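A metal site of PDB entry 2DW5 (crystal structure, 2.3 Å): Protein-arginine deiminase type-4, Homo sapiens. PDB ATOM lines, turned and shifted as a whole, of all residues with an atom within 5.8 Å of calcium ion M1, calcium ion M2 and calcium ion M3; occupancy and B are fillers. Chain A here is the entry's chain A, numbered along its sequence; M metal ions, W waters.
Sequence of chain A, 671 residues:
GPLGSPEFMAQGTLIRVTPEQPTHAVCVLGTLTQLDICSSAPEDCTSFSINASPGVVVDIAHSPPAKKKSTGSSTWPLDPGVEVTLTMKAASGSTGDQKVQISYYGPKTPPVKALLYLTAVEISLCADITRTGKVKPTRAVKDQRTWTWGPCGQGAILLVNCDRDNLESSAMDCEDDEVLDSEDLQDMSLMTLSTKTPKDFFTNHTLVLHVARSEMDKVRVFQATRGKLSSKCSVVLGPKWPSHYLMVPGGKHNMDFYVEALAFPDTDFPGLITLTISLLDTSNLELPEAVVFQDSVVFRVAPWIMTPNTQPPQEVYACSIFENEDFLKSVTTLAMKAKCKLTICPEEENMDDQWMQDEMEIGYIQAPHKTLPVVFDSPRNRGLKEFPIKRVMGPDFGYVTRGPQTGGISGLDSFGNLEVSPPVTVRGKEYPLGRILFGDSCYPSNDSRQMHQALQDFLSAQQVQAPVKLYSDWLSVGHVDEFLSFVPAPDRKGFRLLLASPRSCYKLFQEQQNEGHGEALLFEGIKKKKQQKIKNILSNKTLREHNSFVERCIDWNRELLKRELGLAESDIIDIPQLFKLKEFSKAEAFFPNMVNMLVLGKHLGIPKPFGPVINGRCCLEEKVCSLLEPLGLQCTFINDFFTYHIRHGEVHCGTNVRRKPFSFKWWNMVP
The guanidinium group (NH1) of Arg 220 is in hydrogen-bond range of the backbone carbonyl oxygen (O) of Asp 176, 2.9 Å away. N of Cys 174 sits at hydrogen-bond distance from O of Asn 161 (3.2 Å). The side-chain carboxylate (OE1) of Glu 260 sits at hydrogen-bond distance from the side-chain amide nitrogen (ND2) of Asn 161.
Within 4 Å of calcium ion M1: Asp 173, Asp 176 and Glu 178.
Six residues have an atom within 4 Å of calcium ion M2: Asn 161, Asp 163, Asp 165, Asp 173, Asp 184 and Asp 187. The nearest printed residue that does not touch calcium ion M2 is Arg 164 (5.1 Å).
Of the 25 residues printed, 4 come within 4 Å of calcium ion M3.
Calcium ion M1 is bound by water W2 (2.3 Å), the backbone carbonyl oxygen of Glu 178 (2.3 Å), the side-chain carboxylate of Asp 176 (2.3 Å), the backbone carbonyl oxygen of Asp 173 (2.3 Å) and water W1 (2.7 Å).
Calcium ion M2 is bound by OD2 of Asp 187, OD2 of Asp 173, OD1 of Asp 163, OD1 of Asn 161, OD2 of Asp 184 and OD2 of Asp 165. Calcium ion M2 has six donor atoms within binding distance.
Calcium ion M3 is bound by the side-chain carboxylate (OD1) of Asp 396 (2.3 Å), the side-chain carboxylate (OD2) of Asp 187 (2.5 Å), the side-chain carboxylate (OD2) of Asp 163 (2.7 Å), the side-chain carboxylate (OD1) of Asp 187 (2.7 Å), the side-chain carboxylate (OD1) of Asp 165 (2.7 Å) and the side-chain carboxylate (OD2) of Asp 165 (2.8 Å).
Water W2 lies within hydrogen-bond range of O of Asp 176 (2.6 Å), OE2 of Glu 260 (2.7 Å) and NH1 of Arg 220 (3.3 Å). Water W1 lies within hydrogen-bond range of OE1 of Glu 260 (2.5 Å), OD1 of Asp 184 (2.6 Å) and ND2 of Asn 161 (2.7 Å).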
ATOM      1  N   ASN A 161     -19.082  18.799   3.958  1.00  0.00           N
ATOM      2  CA  ASN A 161     -18.528  18.127   5.134  1.00  0.00           C
ATOM      3  C   ASN A 161     -19.330  18.408   6.410  1.00  0.00           C
ATOM      4  O   ASN A 161     -18.832  18.875   7.427  1.00  0.00           O
ATOM      5  CB  ASN A 161     -17.027  18.397   5.264  1.00  0.00           C
ATOM      6  CG  ASN A 161     -16.300  17.418   6.223  1.00  0.00           C
ATOM      7  OD1 ASN A 161     -16.906  16.486   6.781  1.00  0.00           O
ATOM      8  ND2 ASN A 161     -15.014  17.656   6.423  1.00  0.00           N
ATOM      9  N   CYS A 162     -20.587  17.985   6.359  1.00  0.00           N
ATOM     10  CA  CYS A 162     -21.624  18.412   7.274  1.00  0.00           C
ATOM     11  C   CYS A 162     -21.943  17.375   8.325  1.00  0.00           C
ATOM     12  O   CYS A 162     -22.997  17.456   8.962  1.00  0.00           O
ATOM     13  CB  CYS A 162     -22.898  18.681   6.475  1.00  0.00           C
ATOM     14  SG  CYS A 162     -23.530  17.215   5.661  1.00  0.00           S
ATOM     15  N   ASP A 163     -21.056  16.385   8.473  1.00  0.00           N
ATOM     16  CA  ASP A 163     -21.128  15.428   9.567  1.00  0.00           C
ATOM     17  C   ASP A 163     -20.160  15.844  10.689  1.00  0.00           C
ATOM     18  O   ASP A 163     -19.524  16.905  10.620  1.00  0.00           O
ATOM     19  CB  ASP A 163     -20.887  13.993   9.065  1.00  0.00           C
ATOM     20  CG  ASP A 163     -19.421  13.675   8.796  1.00  0.00           C
ATOM     21  OD1 ASP A 163     -18.615  14.593   8.462  1.00  0.00           O
ATOM     22  OD2 ASP A 163     -19.081  12.464   8.938  1.00  0.00           O
ATOM     23  N   ARG A 164     -20.092  15.012  11.730  1.00  0.00           N
ATOM     24  CA  ARG A 164     -19.325  15.343  12.950  1.00  0.00           C
ATOM     25  C   ARG A 164     -18.530  14.132  13.435  1.00  0.00           C
ATOM     26  O   ARG A 164     -18.976  13.380  14.298  1.00  0.00           O
ATOM     27  CB  ARG A 164     -20.249  15.842  14.063  1.00  0.00           C
ATOM     28  CG  ARG A 164     -19.541  16.438  15.261  1.00  0.00           C
ATOM     29  CD  ARG A 164     -20.504  17.121  16.224  1.00  0.00           C
ATOM     30  NE  ARG A 164     -21.001  16.167  17.211  1.00  0.00           N
ATOM     31  CZ  ARG A 164     -22.285  15.841  17.412  1.00  0.00           C
ATOM     32  NH1 ARG A 164     -23.283  16.396  16.727  1.00  0.00           N
ATOM     33  NH2 ARG A 164     -22.568  14.939  18.338  1.00  0.00           N
ATOM     34  N   ASP A 165     -17.346  13.945  12.841  1.00  0.00           N
ATOM     35  CA  ASP A 165     -16.396  12.917  13.266  1.00  0.00           C
ATOM     36  C   ASP A 165     -15.659  13.300  14.560  1.00  0.00           C
ATOM     37  O   ASP A 165     -15.160  12.424  15.265  1.00  0.00           O
ATOM     38  CB  ASP A 165     -15.356  12.628  12.149  1.00  0.00           C
ATOM     39  CG  ASP A 165     -15.994  12.137  10.849  1.00  0.00           C
ATOM     40  OD1 ASP A 165     -16.757  11.140  10.869  1.00  0.00           O
ATOM     41  OD2 ASP A 165     -15.727  12.768   9.813  1.00  0.00           O
ATOM     42  N   ASP A 173     -17.995  19.255  11.026  1.00  0.00           N
ATOM     43  CA  ASP A 173     -16.533  19.331  10.851  1.00  0.00           C
ATOM     44  C   ASP A 173     -16.077  20.504   9.963  1.00  0.00           C
ATOM     45  O   ASP A 173     -14.981  21.003  10.154  1.00  0.00           O
ATOM     46  CB  ASP A 173     -15.964  18.035  10.275  1.00  0.00           C
ATOM     47  CG  ASP A 173     -16.317  16.787  11.097  1.00  0.00           C
ATOM     48  OD1 ASP A 173     -16.249  16.803  12.355  1.00  0.00           O
ATOM     49  OD2 ASP A 173     -16.652  15.777  10.471  1.00  0.00           O
ATOM     50  N   CYS A 174     -16.906  20.920   8.985  1.00  0.00           N
ATOM     51  CA  CYS A 174     -16.515  21.988   8.049  1.00  0.00           C
ATOM     52  C   CYS A 174     -16.746  23.426   8.536  1.00  0.00           C
ATOM     53  O   CYS A 174     -16.592  24.388   7.775  1.00  0.00           O
ATOM     54  CB  CYS A 174     -17.208  21.817   6.698  1.00  0.00           C
ATOM     55  SG  CYS A 174     -19.000  22.087   6.762  1.00  0.00           S
ATOM     56  N   GLU A 175     -17.089  23.592   9.815  1.00  0.00           N
ATOM     57  CA  GLU A 175     -17.283  24.943  10.331  1.00  0.00           C
ATOM     58  C   GLU A 175     -15.967  25.608  10.800  1.00  0.00           C
ATOM     59  O   GLU A 175     -15.926  26.837  10.935  1.00  0.00           O
ATOM     60  CB  GLU A 175     -18.376  24.950  11.394  1.00  0.00           C
ATOM     61  CG  GLU A 175     -19.761  24.749  10.767  1.00  0.00           C
ATOM     62  CD  GLU A 175     -20.908  24.647  11.775  1.00  0.00           C
ATOM     63  OE1 GLU A 175     -20.645  24.258  12.950  1.00  0.00           O
ATOM     64  OE2 GLU A 175     -22.067  24.946  11.389  1.00  0.00           O
ATOM     65  N   ASP A 176     -14.911  24.819  11.012  1.00  0.00           N
ATOM     66  CA  ASP A 176     -13.581  25.362  11.348  1.00  0.00           C
ATOM     67  C   ASP A 176     -12.673  25.184  10.147  1.00  0.00           C
ATOM     68  O   ASP A 176     -13.105  24.618   9.105  1.00  0.00           O
ATOM     69  CB  ASP A 176     -12.993  24.662  12.583  1.00  0.00           C
ATOM     70  CG  ASP A 176     -12.669  23.185  12.350  1.00  0.00           C
ATOM     71  OD1 ASP A 176     -12.548  22.429  13.335  1.00  0.00           O
ATOM     72  OD2 ASP A 176     -12.523  22.746  11.184  1.00  0.00           O
ATOM     73  N   ASP A 177     -11.424  25.630  10.280  1.00  0.00           N
ATOM     74  CA  ASP A 177     -10.436  25.521   9.178  1.00  0.00           C
ATOM     75  C   ASP A 177      -9.303  24.561   9.518  1.00  0.00           C
ATOM     76  O   ASP A 177      -8.118  24.876   9.348  1.00  0.00           O
ATOM     77  CB  ASP A 177      -9.907  26.896   8.738  1.00  0.00           C
ATOM     78  CG  ASP A 177      -9.956  27.932   9.837  1.00  0.00           C
ATOM     79  OD1 ASP A 177      -9.006  28.010  10.675  1.00  0.00           O
ATOM     80  OD2 ASP A 177     -10.951  28.697   9.855  1.00  0.00           O
ATOM     81  N   GLU A 178      -9.674  23.359   9.968  1.00  0.00           N
ATOM     82  CA  GLU A 178      -8.724  22.338  10.401  1.00  0.00           C
ATOM     83  C   GLU A 178      -9.236  20.920  10.175  1.00  0.00           C
ATOM     84  O   GLU A 178     -10.411  20.633  10.398  1.00  0.00           O
ATOM     85  CB  GLU A 178      -8.487  22.502  11.887  1.00  0.00           C
ATOM     86  CG  GLU A 178      -7.788  23.775  12.247  1.00  0.00           C
ATOM     87  CD  GLU A 178      -7.340  23.760  13.683  1.00  0.00           C
ATOM     88  OE1 GLU A 178      -6.589  22.827  14.060  1.00  0.00           O
ATOM     89  OE2 GLU A 178      -7.736  24.684  14.425  1.00  0.00           O
ATOM     90  N   VAL A 179      -8.336  20.019   9.784  1.00  0.00           N
ATOM     91  CA  VAL A 179      -8.660  18.597   9.763  1.00  0.00           C
ATOM     92  C   VAL A 179      -8.328  18.072  11.165  1.00  0.00           C
ATOM     93  O   VAL A 179      -7.149  17.884  11.480  1.00  0.00           O
ATOM     94  CB  VAL A 179      -7.886  17.822   8.666  1.00  0.00           C
ATOM     95  CG1 VAL A 179      -8.393  16.386   8.567  1.00  0.00           C
ATOM     96  CG2 VAL A 179      -8.045  18.486   7.326  1.00  0.00           C
ATOM     97  N   LEU A 180      -9.344  17.861  11.992  1.00  0.00           N
ATOM     98  CA  LEU A 180      -9.125  17.524  13.428  1.00  0.00           C
ATOM     99  C   LEU A 180      -8.923  16.047  13.666  1.00  0.00           C
ATOM    100  O   LEU A 180      -8.276  15.650  14.628  1.00  0.00           O
ATOM    101  CB  LEU A 180     -10.277  18.006  14.313  1.00  0.00           C
ATOM    102  CG  LEU A 180     -10.277  19.495  14.654  1.00  0.00           C
ATOM    103  CD1 LEU A 180     -11.464  19.788  15.592  1.00  0.00           C
ATOM    104  CD2 LEU A 180      -8.923  19.974  15.237  1.00  0.00           C
ATOM    105  N   GLU A 183      -9.883  10.462  10.225  1.00  0.00           N
ATOM    106  CA  GLU A 183     -11.115   9.944   9.622  1.00  0.00           C
ATOM    107  C   GLU A 183     -11.881  10.986   8.804  1.00  0.00           C
ATOM    108  O   GLU A 183     -12.566  10.640   7.857  1.00  0.00           O
ATOM    109  CB  GLU A 183     -12.079   9.407  10.693  1.00  0.00           C
ATOM    110  CG  GLU A 183     -11.604   8.162  11.410  1.00  0.00           C
ATOM    111  CD  GLU A 183     -10.716   8.470  12.599  1.00  0.00           C
ATOM    112  OE1 GLU A 183     -10.420   7.517  13.346  1.00  0.00           O
ATOM    113  OE2 GLU A 183     -10.309   9.644  12.780  1.00  0.00           O
ATOM    114  N   ASP A 184     -11.772  12.249   9.213  1.00  0.00           N
ATOM    115  CA  ASP A 184     -12.427  13.367   8.551  1.00  0.00           C
ATOM    116  C   ASP A 184     -12.019  13.450   7.076  1.00  0.00           C
ATOM    117  O   ASP A 184     -12.860  13.818   6.220  1.00  0.00           O
ATOM    118  CB  ASP A 184     -12.121  14.699   9.260  1.00  0.00           C
ATOM    119  CG  ASP A 184     -12.870  15.910   8.652  1.00  0.00           C
ATOM    120  OD1 ASP A 184     -12.269  16.995   8.503  1.00  0.00           O
ATOM    121  OD2 ASP A 184     -14.068  15.790   8.328  1.00  0.00           O
ATOM    122  N   GLN A 186     -11.610  11.158   4.995  1.00  0.00           N
ATOM    123  CA  GLN A 186     -12.379  10.226   4.195  1.00  0.00           C
ATOM    124  C   GLN A 186     -13.583  10.895   3.572  1.00  0.00           C
ATOM    125  O   GLN A 186     -14.065  10.456   2.522  1.00  0.00           O
ATOM    126  CB  GLN A 186     -12.814   9.024   5.056  1.00  0.00           C
ATOM    127  CG  GLN A 186     -11.652   8.180   5.583  1.00  0.00           C
ATOM    128  CD  GLN A 186     -12.081   7.161   6.657  1.00  0.00           C
ATOM    129  OE1 GLN A 186     -11.244   6.680   7.447  1.00  0.00           O
ATOM    130  NE2 GLN A 186     -13.381   6.836   6.694  1.00  0.00           N
ATOM    131  N   ASP A 187     -14.093  11.944   4.195  1.00  0.00           N
ATOM    132  CA  ASP A 187     -15.211  12.679   3.599  1.00  0.00           C
ATOM    133  C   ASP A 187     -14.736  13.617   2.511  1.00  0.00           C
ATOM    134  O   ASP A 187     -15.540  14.046   1.698  1.00  0.00           O
ATOM    135  CB  ASP A 187     -15.998  13.478   4.628  1.00  0.00           C
ATOM    136  CG  ASP A 187     -16.537  12.605   5.728  1.00  0.00           C
ATOM    137  OD1 ASP A 187     -16.926  11.433   5.497  1.00  0.00           O
ATOM    138  OD2 ASP A 187     -16.537  13.095   6.859  1.00  0.00           O
ATOM    139  N   MET A 188     -13.433  13.898   2.481  1.00  0.00           N
ATOM    140  CA  MET A 188     -12.876  14.901   1.571  1.00  0.00           C
ATOM    141  C   MET A 188     -12.415  14.318   0.253  1.00  0.00           C
ATOM    142  O   MET A 188     -12.167  13.145   0.155  1.00  0.00           O
ATOM    143  CB  MET A 188     -11.725  15.623   2.257  1.00  0.00           C
ATOM    144  CG  MET A 188     -12.151  16.259   3.523  1.00  0.00           C
ATOM    145  SD  MET A 188     -10.946  17.437   4.109  1.00  0.00           S
ATOM    146  CE  MET A 188     -11.523  17.586   5.784  1.00  0.00           C
ATOM    147  N   ARG A 220     -13.238  24.476   1.055  1.00  0.00           N
ATOM    148  CA  ARG A 220     -11.994  24.605   1.821  1.00  0.00           C
ATOM    149  C   ARG A 220     -11.018  23.559   1.326  1.00  0.00           C
ATOM    150  O   ARG A 220     -11.426  22.449   0.962  1.00  0.00           O
ATOM    151  CB  ARG A 220     -12.248  24.481   3.304  1.00  0.00           C
ATOM    152  CG  ARG A 220     -10.981  24.748   4.118  1.00  0.00           C
ATOM    153  CD  ARG A 220     -11.234  24.717   5.557  1.00  0.00           C
ATOM    154  NE  ARG A 220     -12.029  25.858   5.971  1.00  0.00           N
ATOM    155  CZ  ARG A 220     -13.296  25.822   6.343  1.00  0.00           C
ATOM    156  NH1 ARG A 220     -13.977  24.670   6.379  1.00  0.00           N
ATOM    157  NH2 ARG A 220     -13.902  26.953   6.717  1.00  0.00           N
ATOM    158  N   PHE A 222      -7.166  21.758   1.975  1.00  0.00           N
ATOM    159  CA  PHE A 222      -6.031  21.518   2.864  1.00  0.00           C
ATOM    160  C   PHE A 222      -4.864  20.892   2.085  1.00  0.00           C
ATOM    161  O   PHE A 222      -5.068  20.122   1.159  1.00  0.00           O
ATOM    162  CB  PHE A 222      -6.422  20.557   3.994  1.00  0.00           C
ATOM    163  CG  PHE A 222      -7.536  21.067   4.897  1.00  0.00           C
ATOM    164  CD1 PHE A 222      -8.883  20.804   4.602  1.00  0.00           C
ATOM    165  CD2 PHE A 222      -7.230  21.788   6.047  1.00  0.00           C
ATOM    166  CE1 PHE A 222      -9.916  21.270   5.451  1.00  0.00           C
ATOM    167  CE2 PHE A 222      -8.263  22.257   6.882  1.00  0.00           C
ATOM    168  CZ  PHE A 222      -9.591  21.995   6.586  1.00  0.00           C
ATOM    169  N   GLU A 260     -13.084  19.910   0.756  1.00  0.00           N
ATOM    170  CA  GLU A 260     -14.410  19.686   1.354  1.00  0.00           C
ATOM    171  C   GLU A 260     -15.278  20.804   0.888  1.00  0.00           C
ATOM    172  O   GLU A 260     -14.789  21.917   0.741  1.00  0.00           O
ATOM    173  CB  GLU A 260     -14.322  19.720   2.886  1.00  0.00           C
ATOM    174  CG  GLU A 260     -13.654  20.989   3.497  1.00  0.00           C
ATOM    175  CD  GLU A 260     -13.737  21.007   5.014  1.00  0.00           C
ATOM    176  OE1 GLU A 260     -14.021  19.947   5.609  1.00  0.00           O
ATOM    177  OE2 GLU A 260     -13.524  22.058   5.644  1.00  0.00           O
ATOM    178  N   LYS A 370     -17.146   7.937  -0.952  1.00  0.00           N
ATOM    179  CA  LYS A 370     -17.837   8.077   0.355  1.00  0.00           C
ATOM    180  C   LYS A 370     -19.340   8.387   0.181  1.00  0.00           C
ATOM    181  O   LYS A 370     -19.732   9.295  -0.546  1.00  0.00           O
ATOM    182  CB  LYS A 370     -17.168   9.188   1.208  1.00  0.00           C
ATOM    183  CG  LYS A 370     -17.573   9.210   2.705  1.00  0.00           C
ATOM    184  CD  LYS A 370     -17.075   7.942   3.439  1.00  0.00           C
ATOM    185  CE  LYS A 370     -16.850   8.138   4.952  1.00  0.00           C
ATOM    186  NZ  LYS A 370     -15.679   7.323   5.483  1.00  0.00           N
ATOM    187  N   LEU A 372     -22.690   8.992   2.803  1.00  0.00           N
ATOM    188  CA  LEU A 372     -23.150   9.019   4.196  1.00  0.00           C
ATOM    189  C   LEU A 372     -24.560   9.498   4.371  1.00  0.00           C
ATOM    190  O   LEU A 372     -25.046  10.256   3.555  1.00  0.00           O
ATOM    191  CB  LEU A 372     -22.239   9.840   5.080  1.00  0.00           C
ATOM    192  CG  LEU A 372     -21.879  11.273   4.758  1.00  0.00           C
ATOM    193  CD1 LEU A 372     -21.981  12.143   6.028  1.00  0.00           C
ATOM    194  CD2 LEU A 372     -20.475  11.273   4.252  1.00  0.00           C
ATOM    195  N   PRO A 395     -20.770  10.969  13.896  1.00  0.00           N
ATOM    196  CA  PRO A 395     -19.829  10.244  13.064  1.00  0.00           C
ATOM    197  C   PRO A 395     -20.490   9.554  11.886  1.00  0.00           C
ATOM    198  O   PRO A 395     -21.249   8.605  12.070  1.00  0.00           O
ATOM    199  CB  PRO A 395     -19.218   9.205  14.040  1.00  0.00           C
ATOM    200  CG  PRO A 395     -19.322   9.872  15.374  1.00  0.00           C
ATOM    201  CD  PRO A 395     -20.685  10.534  15.302  1.00  0.00           C
ATOM    202  N   ASP A 396     -20.180  10.067  10.701  1.00  0.00           N
ATOM    203  CA  ASP A 396     -20.736   9.562   9.438  1.00  0.00           C
ATOM    204  C   ASP A 396     -22.245   9.721   9.363  1.00  0.00           C
ATOM    205  O   ASP A 396     -22.956   8.930   8.746  1.00  0.00           O
ATOM    206  CB  ASP A 396     -20.239   8.145   9.112  1.00  0.00           C
ATOM    207  CG  ASP A 396     -18.772   8.143   8.646  1.00  0.00           C
ATOM    208  OD1 ASP A 396     -18.364   9.126   7.998  1.00  0.00           O
ATOM    209  OD2 ASP A 396     -18.013   7.189   8.927  1.00  0.00           O
HETATM  210 CA    CA M   1     -12.683  20.764   9.999  1.00  0.00          CA
HETATM  211 CA    CA M   2     -16.292  14.769   8.410  1.00  0.00          CA
HETATM  212 CA    CA M   3     -17.014  10.996   8.135  1.00  0.00          CA
HETATM  213  O   HOH W   1     -13.431  19.239   7.909  1.00  0.00           O
HETATM  214  O   HOH W   2     -12.672  22.208   8.207  1.00  0.00           O
